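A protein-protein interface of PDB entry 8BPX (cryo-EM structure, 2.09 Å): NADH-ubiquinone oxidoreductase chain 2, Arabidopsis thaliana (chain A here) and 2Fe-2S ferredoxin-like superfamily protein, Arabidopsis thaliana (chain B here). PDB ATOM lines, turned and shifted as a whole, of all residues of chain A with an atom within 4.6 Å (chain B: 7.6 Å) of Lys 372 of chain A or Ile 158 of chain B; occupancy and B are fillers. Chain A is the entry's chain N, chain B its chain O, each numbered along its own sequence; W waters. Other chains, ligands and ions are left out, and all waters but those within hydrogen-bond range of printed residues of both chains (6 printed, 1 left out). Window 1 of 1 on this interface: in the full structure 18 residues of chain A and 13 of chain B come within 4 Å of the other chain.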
ATOM      1  N   PHE A 171      17.304  -3.905 -25.378  1.00  0.00           N
ATOM      2  CA  PHE A 171      17.679  -5.259 -24.908  1.00  0.00           C
ATOM      3  C   PHE A 171      17.812  -6.208 -26.111  1.00  0.00           C
ATOM      4  O   PHE A 171      18.829  -6.892 -26.223  1.00  0.00           O
ATOM      5  CB  PHE A 171      16.680  -5.736 -23.849  1.00  0.00           C
ATOM      6  CG  PHE A 171      16.608  -4.868 -22.620  1.00  0.00           C
ATOM      7  CD1 PHE A 171      17.669  -4.810 -21.733  1.00  0.00           C
ATOM      8  CD2 PHE A 171      15.483  -4.102 -22.354  1.00  0.00           C
ATOM      9  CE1 PHE A 171      17.605  -4.012 -20.602  1.00  0.00           C
ATOM     10  CE2 PHE A 171      15.419  -3.308 -21.220  1.00  0.00           C
ATOM     11  CZ  PHE A 171      16.479  -3.265 -20.347  1.00  0.00           C
ATOM     12  N   GLU A 255      18.272 -13.505 -21.877  1.00  0.00           N
ATOM     13  CA  GLU A 255      17.469 -12.462 -21.204  1.00  0.00           C
ATOM     14  C   GLU A 255      16.997 -11.436 -22.243  1.00  0.00           C
ATOM     15  O   GLU A 255      15.815 -11.092 -22.208  1.00  0.00           O
ATOM     16  CB  GLU A 255      18.269 -11.799 -20.089  1.00  0.00           C
ATOM     17  CG  GLU A 255      17.583 -10.561 -19.565  1.00  0.00           C
ATOM     18  CD  GLU A 255      18.165 -10.026 -18.278  1.00  0.00           C
ATOM     19  OE1 GLU A 255      19.391  -9.908 -18.202  1.00  0.00           O
ATOM     20  OE2 GLU A 255      17.389  -9.741 -17.367  1.00  0.00           O
ATOM     21  N   LYS A 314      16.391 -12.223 -11.249  1.00  0.00           N
ATOM     22  CA  LYS A 314      15.421 -12.225 -12.335  1.00  0.00           C
ATOM     23  C   LYS A 314      15.214 -13.642 -12.858  1.00  0.00           C
ATOM     24  O   LYS A 314      16.135 -14.461 -12.869  1.00  0.00           O
ATOM     25  CB  LYS A 314      15.867 -11.299 -13.467  1.00  0.00           C
ATOM     26  CG  LYS A 314      16.020  -9.851 -13.029  1.00  0.00           C
ATOM     27  CD  LYS A 314      16.246  -8.938 -14.213  1.00  0.00           C
ATOM     28  CE  LYS A 314      17.718  -8.632 -14.389  1.00  0.00           C
ATOM     29  NZ  LYS A 314      17.961  -7.845 -15.628  1.00  0.00           N
ATOM     30  N   VAL A 315      13.985 -13.915 -13.304  1.00  0.00           N
ATOM     31  CA  VAL A 315      13.577 -15.281 -13.623  1.00  0.00           C
ATOM     32  C   VAL A 315      14.356 -15.821 -14.821  1.00  0.00           C
ATOM     33  O   VAL A 315      14.901 -16.933 -14.778  1.00  0.00           O
ATOM     34  CB  VAL A 315      12.058 -15.337 -13.864  1.00  0.00           C
ATOM     35  CG1 VAL A 315      11.614 -16.756 -14.175  1.00  0.00           C
ATOM     36  CG2 VAL A 315      11.303 -14.783 -12.657  1.00  0.00           C
ATOM     37  N   LYS A 316      14.378 -15.048 -15.908  1.00  0.00           N
ATOM     38  CA  LYS A 316      15.027 -15.515 -17.166  1.00  0.00           C
ATOM     39  C   LYS A 316      16.513 -15.835 -16.923  1.00  0.00           C
ATOM     40  O   LYS A 316      16.946 -16.901 -17.359  1.00  0.00           O
ATOM     41  CB  LYS A 316      14.880 -14.486 -18.285  1.00  0.00           C
ATOM     42  CG  LYS A 316      13.511 -14.413 -18.937  1.00  0.00           C
ATOM     43  CD  LYS A 316      13.502 -13.439 -20.083  1.00  0.00           C
ATOM     44  CE  LYS A 316      13.508 -14.125 -21.429  1.00  0.00           C
ATOM     45  NZ  LYS A 316      13.612 -13.148 -22.534  1.00  0.00           N
ATOM     46  N   ARG A 367       4.215 -13.560 -18.518  1.00  0.00           N
ATOM     47  CA  ARG A 367       4.738 -12.382 -19.269  1.00  0.00           C
ATOM     48  C   ARG A 367       3.581 -11.512 -19.770  1.00  0.00           C
ATOM     49  O   ARG A 367       3.828 -10.349 -20.112  1.00  0.00           O
ATOM     50  CB  ARG A 367       5.616 -12.801 -20.451  1.00  0.00           C
ATOM     51  CG  ARG A 367       7.051 -13.122 -20.059  1.00  0.00           C
ATOM     52  CD  ARG A 367       7.750 -11.919 -19.462  1.00  0.00           C
ATOM     53  NE  ARG A 367       7.871 -10.851 -20.444  1.00  0.00           N
ATOM     54  CZ  ARG A 367       8.164  -9.589 -20.158  1.00  0.00           C
ATOM     55  NH1 ARG A 367       8.379  -9.225 -18.905  1.00  0.00           N
ATOM     56  NH2 ARG A 367       8.242  -8.698 -21.128  1.00  0.00           N
ATOM     57  N   ARG A 370       3.921  -9.057 -17.476  1.00  0.00           N
ATOM     58  CA  ARG A 370       5.281  -8.517 -17.460  1.00  0.00           C
ATOM     59  C   ARG A 370       6.075  -8.966 -16.232  1.00  0.00           C
ATOM     60  O   ARG A 370       6.687  -8.155 -15.536  1.00  0.00           O
ATOM     61  CB  ARG A 370       5.259  -6.990 -17.557  1.00  0.00           C
ATOM     62  CG  ARG A 370       4.841  -6.454 -18.900  1.00  0.00           C
ATOM     63  CD  ARG A 370       5.986  -6.536 -19.888  1.00  0.00           C
ATOM     64  NE  ARG A 370       5.616  -6.055 -21.214  1.00  0.00           N
ATOM     65  CZ  ARG A 370       4.802  -6.690 -22.045  1.00  0.00           C
ATOM     66  NH1 ARG A 370       4.266  -7.858 -21.733  1.00  0.00           N
ATOM     67  NH2 ARG A 370       4.527  -6.142 -23.225  1.00  0.00           N
ATOM     68  N   VAL A 371       6.074 -10.275 -15.970  1.00  0.00           N
ATOM     69  CA  VAL A 371       6.905 -10.797 -14.892  1.00  0.00           C
ATOM     70  C   VAL A 371       8.369 -10.544 -15.224  1.00  0.00           C
ATOM     71  O   VAL A 371       8.826 -10.798 -16.346  1.00  0.00           O
ATOM     72  CB  VAL A 371       6.613 -12.287 -14.643  1.00  0.00           C
ATOM     73  CG1 VAL A 371       7.097 -13.157 -15.795  1.00  0.00           C
ATOM     74  CG2 VAL A 371       7.240 -12.732 -13.334  1.00  0.00           C
ATOM     75  N   LYS A 372       9.133 -10.045 -14.261  1.00  0.00           N
ATOM     76  CA  LYS A 372      10.574  -9.770 -14.511  1.00  0.00           C
ATOM     77  C   LYS A 372      11.405 -10.313 -13.349  1.00  0.00           C
ATOM     78  O   LYS A 372      12.411 -10.975 -13.610  1.00  0.00           O
ATOM     79  CB  LYS A 372      10.805  -8.271 -14.717  1.00  0.00           C
ATOM     80  CG  LYS A 372      12.214  -7.848 -15.097  1.00  0.00           C
ATOM     81  CD  LYS A 372      12.309  -6.353 -15.305  1.00  0.00           C
ATOM     82  CE  LYS A 372      13.709  -5.816 -15.128  1.00  0.00           C
ATOM     83  NZ  LYS A 372      13.761  -4.343 -15.276  1.00  0.00           N
ATOM     84  N   TYR A 373      10.972 -10.039 -12.123  1.00  0.00           N
ATOM     85  CA  TYR A 373      11.764 -10.394 -10.959  1.00  0.00           C
ATOM     86  C   TYR A 373      11.163 -11.606 -10.258  1.00  0.00           C
ATOM     87  O   TYR A 373       9.960 -11.858 -10.346  1.00  0.00           O
ATOM     88  CB  TYR A 373      11.845  -9.230  -9.967  1.00  0.00           C
ATOM     89  CG  TYR A 373      12.485  -7.972 -10.514  1.00  0.00           C
ATOM     90  CD1 TYR A 373      13.866  -7.814 -10.511  1.00  0.00           C
ATOM     91  CD2 TYR A 373      11.706  -6.937 -11.013  1.00  0.00           C
ATOM     92  CE1 TYR A 373      14.454  -6.663 -11.003  1.00  0.00           C
ATOM     93  CE2 TYR A 373      12.284  -5.784 -11.506  1.00  0.00           C
ATOM     94  CZ  TYR A 373      13.658  -5.651 -11.499  1.00  0.00           C
ATOM     95  OH  TYR A 373      14.237  -4.504 -11.986  1.00  0.00           O
ATOM     96  N   ILE A 374      12.017 -12.345  -9.553  1.00  0.00           N
ATOM     97  CA  ILE A 374      11.536 -13.447  -8.726  1.00  0.00           C
ATOM     98  C   ILE A 374      10.536 -12.937  -7.696  1.00  0.00           C
ATOM     99  O   ILE A 374       9.506 -13.572  -7.443  1.00  0.00           O
ATOM    100  CB  ILE A 374      12.719 -14.176  -8.063  1.00  0.00           C
ATOM    101  CG1 ILE A 374      13.523 -14.955  -9.107  1.00  0.00           C
ATOM    102  CG2 ILE A 374      12.232 -15.105  -6.961  1.00  0.00           C
ATOM    103  CD1 ILE A 374      14.969 -15.167  -8.722  1.00  0.00           C
ATOM    104  N   ASP A 376       8.405 -10.717  -8.021  1.00  0.00           N
ATOM    105  CA  ASP A 376       7.100 -10.491  -8.636  1.00  0.00           C
ATOM    106  C   ASP A 376       6.158 -11.678  -8.452  1.00  0.00           C
ATOM    107  O   ASP A 376       4.950 -11.530  -8.651  1.00  0.00           O
ATOM    108  CB  ASP A 376       7.253 -10.189 -10.130  1.00  0.00           C
ATOM    109  CG  ASP A 376       7.927  -8.856 -10.402  1.00  0.00           C
ATOM    110  OD1 ASP A 376       7.882  -7.966  -9.523  1.00  0.00           O
ATOM    111  OD2 ASP A 376       8.504  -8.695 -11.499  1.00  0.00           O
ATOM    112  N   ALA B  81       4.652   1.499 -14.137  1.00  0.00           N
ATOM    113  CA  ALA B  81       4.825   0.159 -14.684  1.00  0.00           C
ATOM    114  C   ALA B  81       6.273  -0.312 -14.632  1.00  0.00           C
ATOM    115  O   ALA B  81       6.519  -1.520 -14.634  1.00  0.00           O
ATOM    116  CB  ALA B  81       4.318   0.115 -16.127  1.00  0.00           C
ATOM    117  N   SER B  82       7.233   0.612 -14.589  1.00  0.00           N
ATOM    118  CA  SER B  82       8.639   0.233 -14.571  1.00  0.00           C
ATOM    119  C   SER B  82       9.125  -0.185 -13.190  1.00  0.00           C
ATOM    120  O   SER B  82      10.192  -0.794 -13.085  1.00  0.00           O
ATOM    121  CB  SER B  82       9.499   1.387 -15.088  1.00  0.00           C
ATOM    122  OG  SER B  82       9.736   2.342 -14.069  1.00  0.00           O
ATOM    123  N   ARG B  84       7.018  -1.629  -9.932  1.00  0.00           N
ATOM    124  CA  ARG B  84       5.695  -1.886  -9.377  1.00  0.00           C
ATOM    125  C   ARG B  84       5.718  -2.246  -7.900  1.00  0.00           C
ATOM    126  O   ARG B  84       4.698  -2.076  -7.224  1.00  0.00           O
ATOM    127  CB  ARG B  84       4.999  -2.995 -10.171  1.00  0.00           C
ATOM    128  CG  ARG B  84       4.317  -2.485 -11.436  1.00  0.00           C
ATOM    129  CD  ARG B  84       3.665  -3.597 -12.235  1.00  0.00           C
ATOM    130  NE  ARG B  84       4.633  -4.569 -12.724  1.00  0.00           N
ATOM    131  CZ  ARG B  84       4.312  -5.706 -13.324  1.00  0.00           C
ATOM    132  NH1 ARG B  84       3.051  -6.037 -13.546  1.00  0.00           N
ATOM    133  NH2 ARG B  84       5.280  -6.526 -13.719  1.00  0.00           N
ATOM    134  N   GLU B  89      14.676  -6.111  -3.930  1.00  0.00           N
ATOM    135  CA  GLU B  89      14.854  -7.298  -4.757  1.00  0.00           C
ATOM    136  C   GLU B  89      14.171  -7.184  -6.115  1.00  0.00           C
ATOM    137  O   GLU B  89      14.405  -8.032  -6.980  1.00  0.00           O
ATOM    138  CB  GLU B  89      14.332  -8.532  -4.021  1.00  0.00           C
ATOM    139  CG  GLU B  89      14.966  -8.757  -2.664  1.00  0.00           C
ATOM    140  CD  GLU B  89      14.495 -10.037  -2.010  1.00  0.00           C
ATOM    141  OE1 GLU B  89      14.808 -11.126  -2.536  1.00  0.00           O
ATOM    142  OE2 GLU B  89      13.808  -9.957  -0.970  1.00  0.00           O
ATOM    143  N   ALA B  90      13.341  -6.171  -6.324  1.00  0.00           N
ATOM    144  CA  ALA B  90      12.694  -5.928  -7.607  1.00  0.00           C
ATOM    145  C   ALA B  90      13.105  -4.569  -8.160  1.00  0.00           C
ATOM    146  O   ALA B  90      12.280  -3.803  -8.661  1.00  0.00           O
ATOM    147  CB  ALA B  90      11.176  -6.029  -7.480  1.00  0.00           C
ATOM    148  N   CYS B  91      14.394  -4.255  -8.072  1.00  0.00           N
ATOM    149  CA  CYS B  91      14.895  -2.928  -8.404  1.00  0.00           C
ATOM    150  C   CYS B  91      16.115  -3.034  -9.306  1.00  0.00           C
ATOM    151  O   CYS B  91      17.079  -3.729  -8.976  1.00  0.00           O
ATOM    152  CB  CYS B  91      15.251  -2.144  -7.134  1.00  0.00           C
ATOM    153  SG  CYS B  91      16.058  -0.557  -7.446  1.00  0.00           S
ATOM    154  N   SER B  92      16.073  -2.329 -10.432  1.00  0.00           N
ATOM    155  CA  SER B  92      17.230  -2.134 -11.295  1.00  0.00           C
ATOM    156  C   SER B  92      17.519  -0.645 -11.454  1.00  0.00           C
ATOM    157  O   SER B  92      17.874  -0.172 -12.534  1.00  0.00           O
ATOM    158  CB  SER B  92      17.025  -2.803 -12.653  1.00  0.00           C
ATOM    159  OG  SER B  92      17.008  -4.214 -12.533  1.00  0.00           O
ATOM    160  N   ALA B  93      17.344   0.104 -10.365  1.00  0.00           N
ATOM    161  CA  ALA B  93      17.587   1.547 -10.292  1.00  0.00           C
ATOM    162  C   ALA B  93      16.686   2.348 -11.227  1.00  0.00           C
ATOM    163  O   ALA B  93      17.028   3.471 -11.608  1.00  0.00           O
ATOM    164  CB  ALA B  93      19.058   1.885 -10.556  1.00  0.00           C
ATOM    165  N   GLU B  94      15.531   1.797 -11.604  1.00  0.00           N
ATOM    166  CA  GLU B  94      14.529   2.597 -12.298  1.00  0.00           C
ATOM    167  C   GLU B  94      14.010   3.733 -11.426  1.00  0.00           C
ATOM    168  O   GLU B  94      13.540   4.744 -11.954  1.00  0.00           O
ATOM    169  CB  GLU B  94      13.366   1.712 -12.755  1.00  0.00           C
ATOM    170  CG  GLU B  94      13.759   0.594 -13.708  1.00  0.00           C
ATOM    171  CD  GLU B  94      14.104  -0.695 -12.986  1.00  0.00           C
ATOM    172  OE1 GLU B  94      14.229  -0.673 -11.744  1.00  0.00           O
ATOM    173  OE2 GLU B  94      14.246  -1.731 -13.661  1.00  0.00           O
ATOM    174  N   PRO B 155      16.213   1.875 -19.835  1.00  0.00           N
ATOM    175  CA  PRO B 155      15.362   0.792 -20.398  1.00  0.00           C
ATOM    176  C   PRO B 155      15.050  -0.211 -19.281  1.00  0.00           C
ATOM    177  O   PRO B 155      15.895  -0.558 -18.481  1.00  0.00           O
ATOM    178  CB  PRO B 155      16.191   0.169 -21.537  1.00  0.00           C
ATOM    179  CG  PRO B 155      17.574   0.535 -21.115  1.00  0.00           C
ATOM    180  CD  PRO B 155      17.462   1.954 -20.610  1.00  0.00           C
ATOM    181  N   TRP B 156      13.820  -0.709 -19.281  1.00  0.00           N
ATOM    182  CA  TRP B 156      13.395  -1.564 -18.145  1.00  0.00           C
ATOM    183  C   TRP B 156      12.632  -2.802 -18.632  1.00  0.00           C
ATOM    184  O   TRP B 156      12.571  -3.786 -17.881  1.00  0.00           O
ATOM    185  CB  TRP B 156      12.584  -0.730 -17.141  1.00  0.00           C
ATOM    186  CG  TRP B 156      11.320  -0.156 -17.696  1.00  0.00           C
ATOM    187  CD1 TRP B 156      11.151   1.088 -18.227  1.00  0.00           C
ATOM    188  CD2 TRP B 156      10.041  -0.808 -17.782  1.00  0.00           C
ATOM    189  NE1 TRP B 156       9.857   1.255 -18.637  1.00  0.00           N
ATOM    190  CE2 TRP B 156       9.152   0.109 -18.379  1.00  0.00           C
ATOM    191  CE3 TRP B 156       9.559  -2.068 -17.407  1.00  0.00           C
ATOM    192  CZ2 TRP B 156       7.812  -0.195 -18.608  1.00  0.00           C
ATOM    193  CZ3 TRP B 156       8.237  -2.371 -17.642  1.00  0.00           C
ATOM    194  CH2 TRP B 156       7.378  -1.445 -18.234  1.00  0.00           C
ATOM    195  N   ASP B 157      12.039  -2.726 -19.816  1.00  0.00           N
ATOM    196  CA  ASP B 157      10.988  -3.673 -20.264  1.00  0.00           C
ATOM    197  C   ASP B 157      11.637  -4.807 -21.069  1.00  0.00           C
ATOM    198  O   ASP B 157      11.585  -4.789 -22.290  1.00  0.00           O
ATOM    199  CB  ASP B 157       9.873  -2.950 -21.021  1.00  0.00           C
ATOM    200  CG  ASP B 157       8.651  -3.816 -21.274  1.00  0.00           C
ATOM    201  OD1 ASP B 157       7.784  -3.384 -22.049  1.00  0.00           O
ATOM    202  OD2 ASP B 157       8.580  -4.915 -20.699  1.00  0.00           O
ATOM    203  N   ILE B 158      12.189  -5.780 -20.354  1.00  0.00           N
ATOM    204  CA  ILE B 158      12.904  -6.955 -20.930  1.00  0.00           C
ATOM    205  C   ILE B 158      11.956  -7.686 -21.887  1.00  0.00           C
ATOM    206  O   ILE B 158      10.836  -8.007 -21.479  1.00  0.00           O
ATOM    207  CB  ILE B 158      13.416  -7.850 -19.781  1.00  0.00           C
ATOM    208  CG1 ILE B 158      14.801  -7.429 -19.281  1.00  0.00           C
ATOM    209  CG2 ILE B 158      13.411  -9.321 -20.173  1.00  0.00           C
ATOM    210  CD1 ILE B 158      14.888  -6.034 -18.726  1.00  0.00           C
ATOM    211  N   PRO B 159      12.339  -7.892 -23.167  1.00  0.00           N
ATOM    212  CA  PRO B 159      11.562  -8.718 -24.102  1.00  0.00           C
ATOM    213  C   PRO B 159      11.203 -10.100 -23.528  1.00  0.00           C
ATOM    214  O   PRO B 159      12.100 -10.777 -23.071  1.00  0.00           O
ATOM    215  CB  PRO B 159      12.534  -8.870 -25.276  1.00  0.00           C
ATOM    216  CG  PRO B 159      13.299  -7.574 -25.270  1.00  0.00           C
ATOM    217  CD  PRO B 159      13.526  -7.312 -23.797  1.00  0.00           C
HETATM  218  O   HOH W   1      16.759  -4.710 -15.570  1.00  0.00           O
HETATM  219  O   HOH W   2       8.020  -6.294 -12.864  1.00  0.00           O
HETATM  220  O   HOH W   3       9.515  -6.663 -18.362  1.00  0.00           O
HETATM  221  O   HOH W   4      11.470  -3.123 -13.969  1.00  0.00           O
HETATM  222  O   HOH W   5      13.800 -10.844  -7.151  1.00  0.00           O
HETATM  223  O   HOH W   6       4.941  -9.212 -12.794  1.00  0.00           O
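The side-chain amino group (NZ) of Lys 316 of chain A is in hydrogen-bond range of the backbone carbonyl oxygen (O) of Pro 159 of chain B, 2.9 Å away. The guanidinium group of Arg 367 of chain A is in salt-bridge range of the side-chain carboxylate of Asp 157 of chain B, at 3.8 Å. NH2 of Arg 367 of chain A lies within hydrogen-bond range of O of Ile 158 of chain B, 2.7 Å away. O of Arg 370 of chain A lies within hydrogen-bond range of NH2 of Arg 84 of chain B, at 2.8 Å. The guanidinium group (NE) of Arg 370 of chain A lies within salt-bridge range of the side-chain carboxylate (OD2) of Asp 157 of chain B (3.2 Å). The side-chain carboxylate (OE2) of Glu 94 of chain B is in salt-bridge range of the side-chain amino group (NZ) of Lys 372 of chain A, 3.1 Å away. The side-chain amino group (NZ) of Lys 372 of chain A is in hydrogen-bond range of the backbone carbonyl oxygen (O) of Trp 156 of chain B (2.9 Å). The side-chain hydroxyl of Tyr 373 of chain A sits at hydrogen-bond distance from the side-chain hydroxyl of Ser 92 of chain B, at 2.8 Å. The side-chain carboxylate (OE2) of Glu 94 of chain B is in hydrogen-bond range of the side-chain hydroxyl (OH) of Tyr 373 of chain A, 3.2 Å away.
OE2 of Glu 255 of chain A lies within salt-bridge range of NZ of Lys 314 of chain A (2.6 Å). The backbone NH (N) of Val 315 of chain A is in hydrogen-bond range of the backbone carbonyl oxygen (O) of Lys 372 of chain A (3.3 Å). The side-chain amino group of Lys 372 of chain A is in hydrogen-bond range of the side-chain hydroxyl of Tyr 373 of chain A (3.3 Å). The backbone NH of Lys 372 of chain A sits at hydrogen-bond distance from the side-chain carboxylate of Asp 376 of chain A (3.1 Å). The side-chain carboxylate (OD2) of Asp 376 of chain A sits at hydrogen-bond distance from the backbone NH (N) of Tyr 373 of chain A (2.9 Å). SG of Cys 91 of chain B lies close to N of Ala 93 of chain B (3.3 Å).
Among the printed residues, pairs that only touch across the chains: Phe 171 of chain A with Pro 155 of chain B, Phe 171 of chain A with Trp 156 of chain B, Phe 171 of chain A with Asp 157 of chain B, Phe 171 of chain A with Ile 158 of chain B, Phe 171 of chain A with Pro 159 of chain B, Glu 255 of chain A with Ile 158 of chain B, Glu 255 of chain A with Pro 159 of chain B, Lys 372 of chain A with Ile 158 of chain B, Tyr 373 of chain A with Glu 89 of chain B, Tyr 373 of chain A with Ala 90 of chain B and Tyr 373 of chain A with Cys 91 of chain B.
Of the printed residues of chain B, Lys 316 of chain A touches Pro 159. Lys 372 of chain A touches just these residues of chain B: Glu 94 (3.1 Å), Trp 156 (2.9 Å) and Ile 158 (3.8 Å). Of the printed residues of chain B, Tyr 373 of chain A touches Glu 89 (3.6 Å), Ala 90 (3.5 Å), Cys 91 (3.6 Å), Ser 92 (2.8 Å) and Glu 94 (3.2 Å). Ile 374 of chain A touches none of the printed residues of chain B. Ala 93 of chain B touches none of the printed residues of chain A. Printed residues of chain A within 4 Å of Glu 94 of chain B: Lys 372 and Tyr 373. Ile 158 of chain B touches just these residues of chain A: Phe 171 (3.6 Å), Glu 255 (3.6 Å), Arg 367 (2.7 Å) and Lys 372 (3.8 Å). Of the printed residues of chain A, Pro 159 of chain B touches Phe 171, Glu 255 and Lys 316. The nearest printed residue of chain B that does not touch Glu 255 of chain A is Ser 92 of chain B (7.4 Å).
Hydrophobic or aromatic side chains of chain B within 4 Å of the printed part of chain A: Ala 90, Pro 155, Ile 158 and Pro 159. Of the 12 printed residues of chain A, 7 touch a printed residue of chain B. Printed residues of chain A that touch a printed residue of chain B: Phe 171, Glu 255, Lys 316, Arg 367, Arg 370, Lys 372 and Tyr 373. Among the printed residues, 20 pairs touch across the chains. Among the printed residues, Asp or Glu carboxylates within 4 Å of a Lys or Arg side-chain nitrogen of the other chain: Arg 367 of chain A with Asp 157 of chain B (3.8 Å), Arg 370 of chain A with Asp 157 of chain B (3.2 Å) and Lys 372 of chain A with Glu 94 of chain B (3.1 Å).
Water W4 lies within hydrogen-bond range of O of Ser 82 of chain B (2.8 Å), NZ of Lys 372 of chain A (2.9 Å) and OE2 of Glu 94 of chain B (3.1 Å). Water W2 bridges the side-chain carboxylate (OD2) of Asp 376 of chain A and the guanidinium group (NH2) of Arg 84 of chain B. Water W3 lies within hydrogen-bond range of NH1 of Arg 367 of chain A (2.9 Å), OD2 of Asp 157 of chain B (3.1 Å) and N of Ile 158 of chain B (3.4 Å). Water W6 lies within hydrogen-bond range of NH2 of Arg 84 of chain B and O of Arg 370 of chain A. Water W5 lies within hydrogen-bond range of O of Glu 89 of chain B and N of Ile 374 of chain A. Water W1 lies within hydrogen-bond range of the side-chain amino group of Lys 372 of chain A (3.0 Å), the side-chain hydroxyl of Ser 92 of chain B (3.1 Å) and the side-chain amino group of Lys 314 of chain A (3.4 Å).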
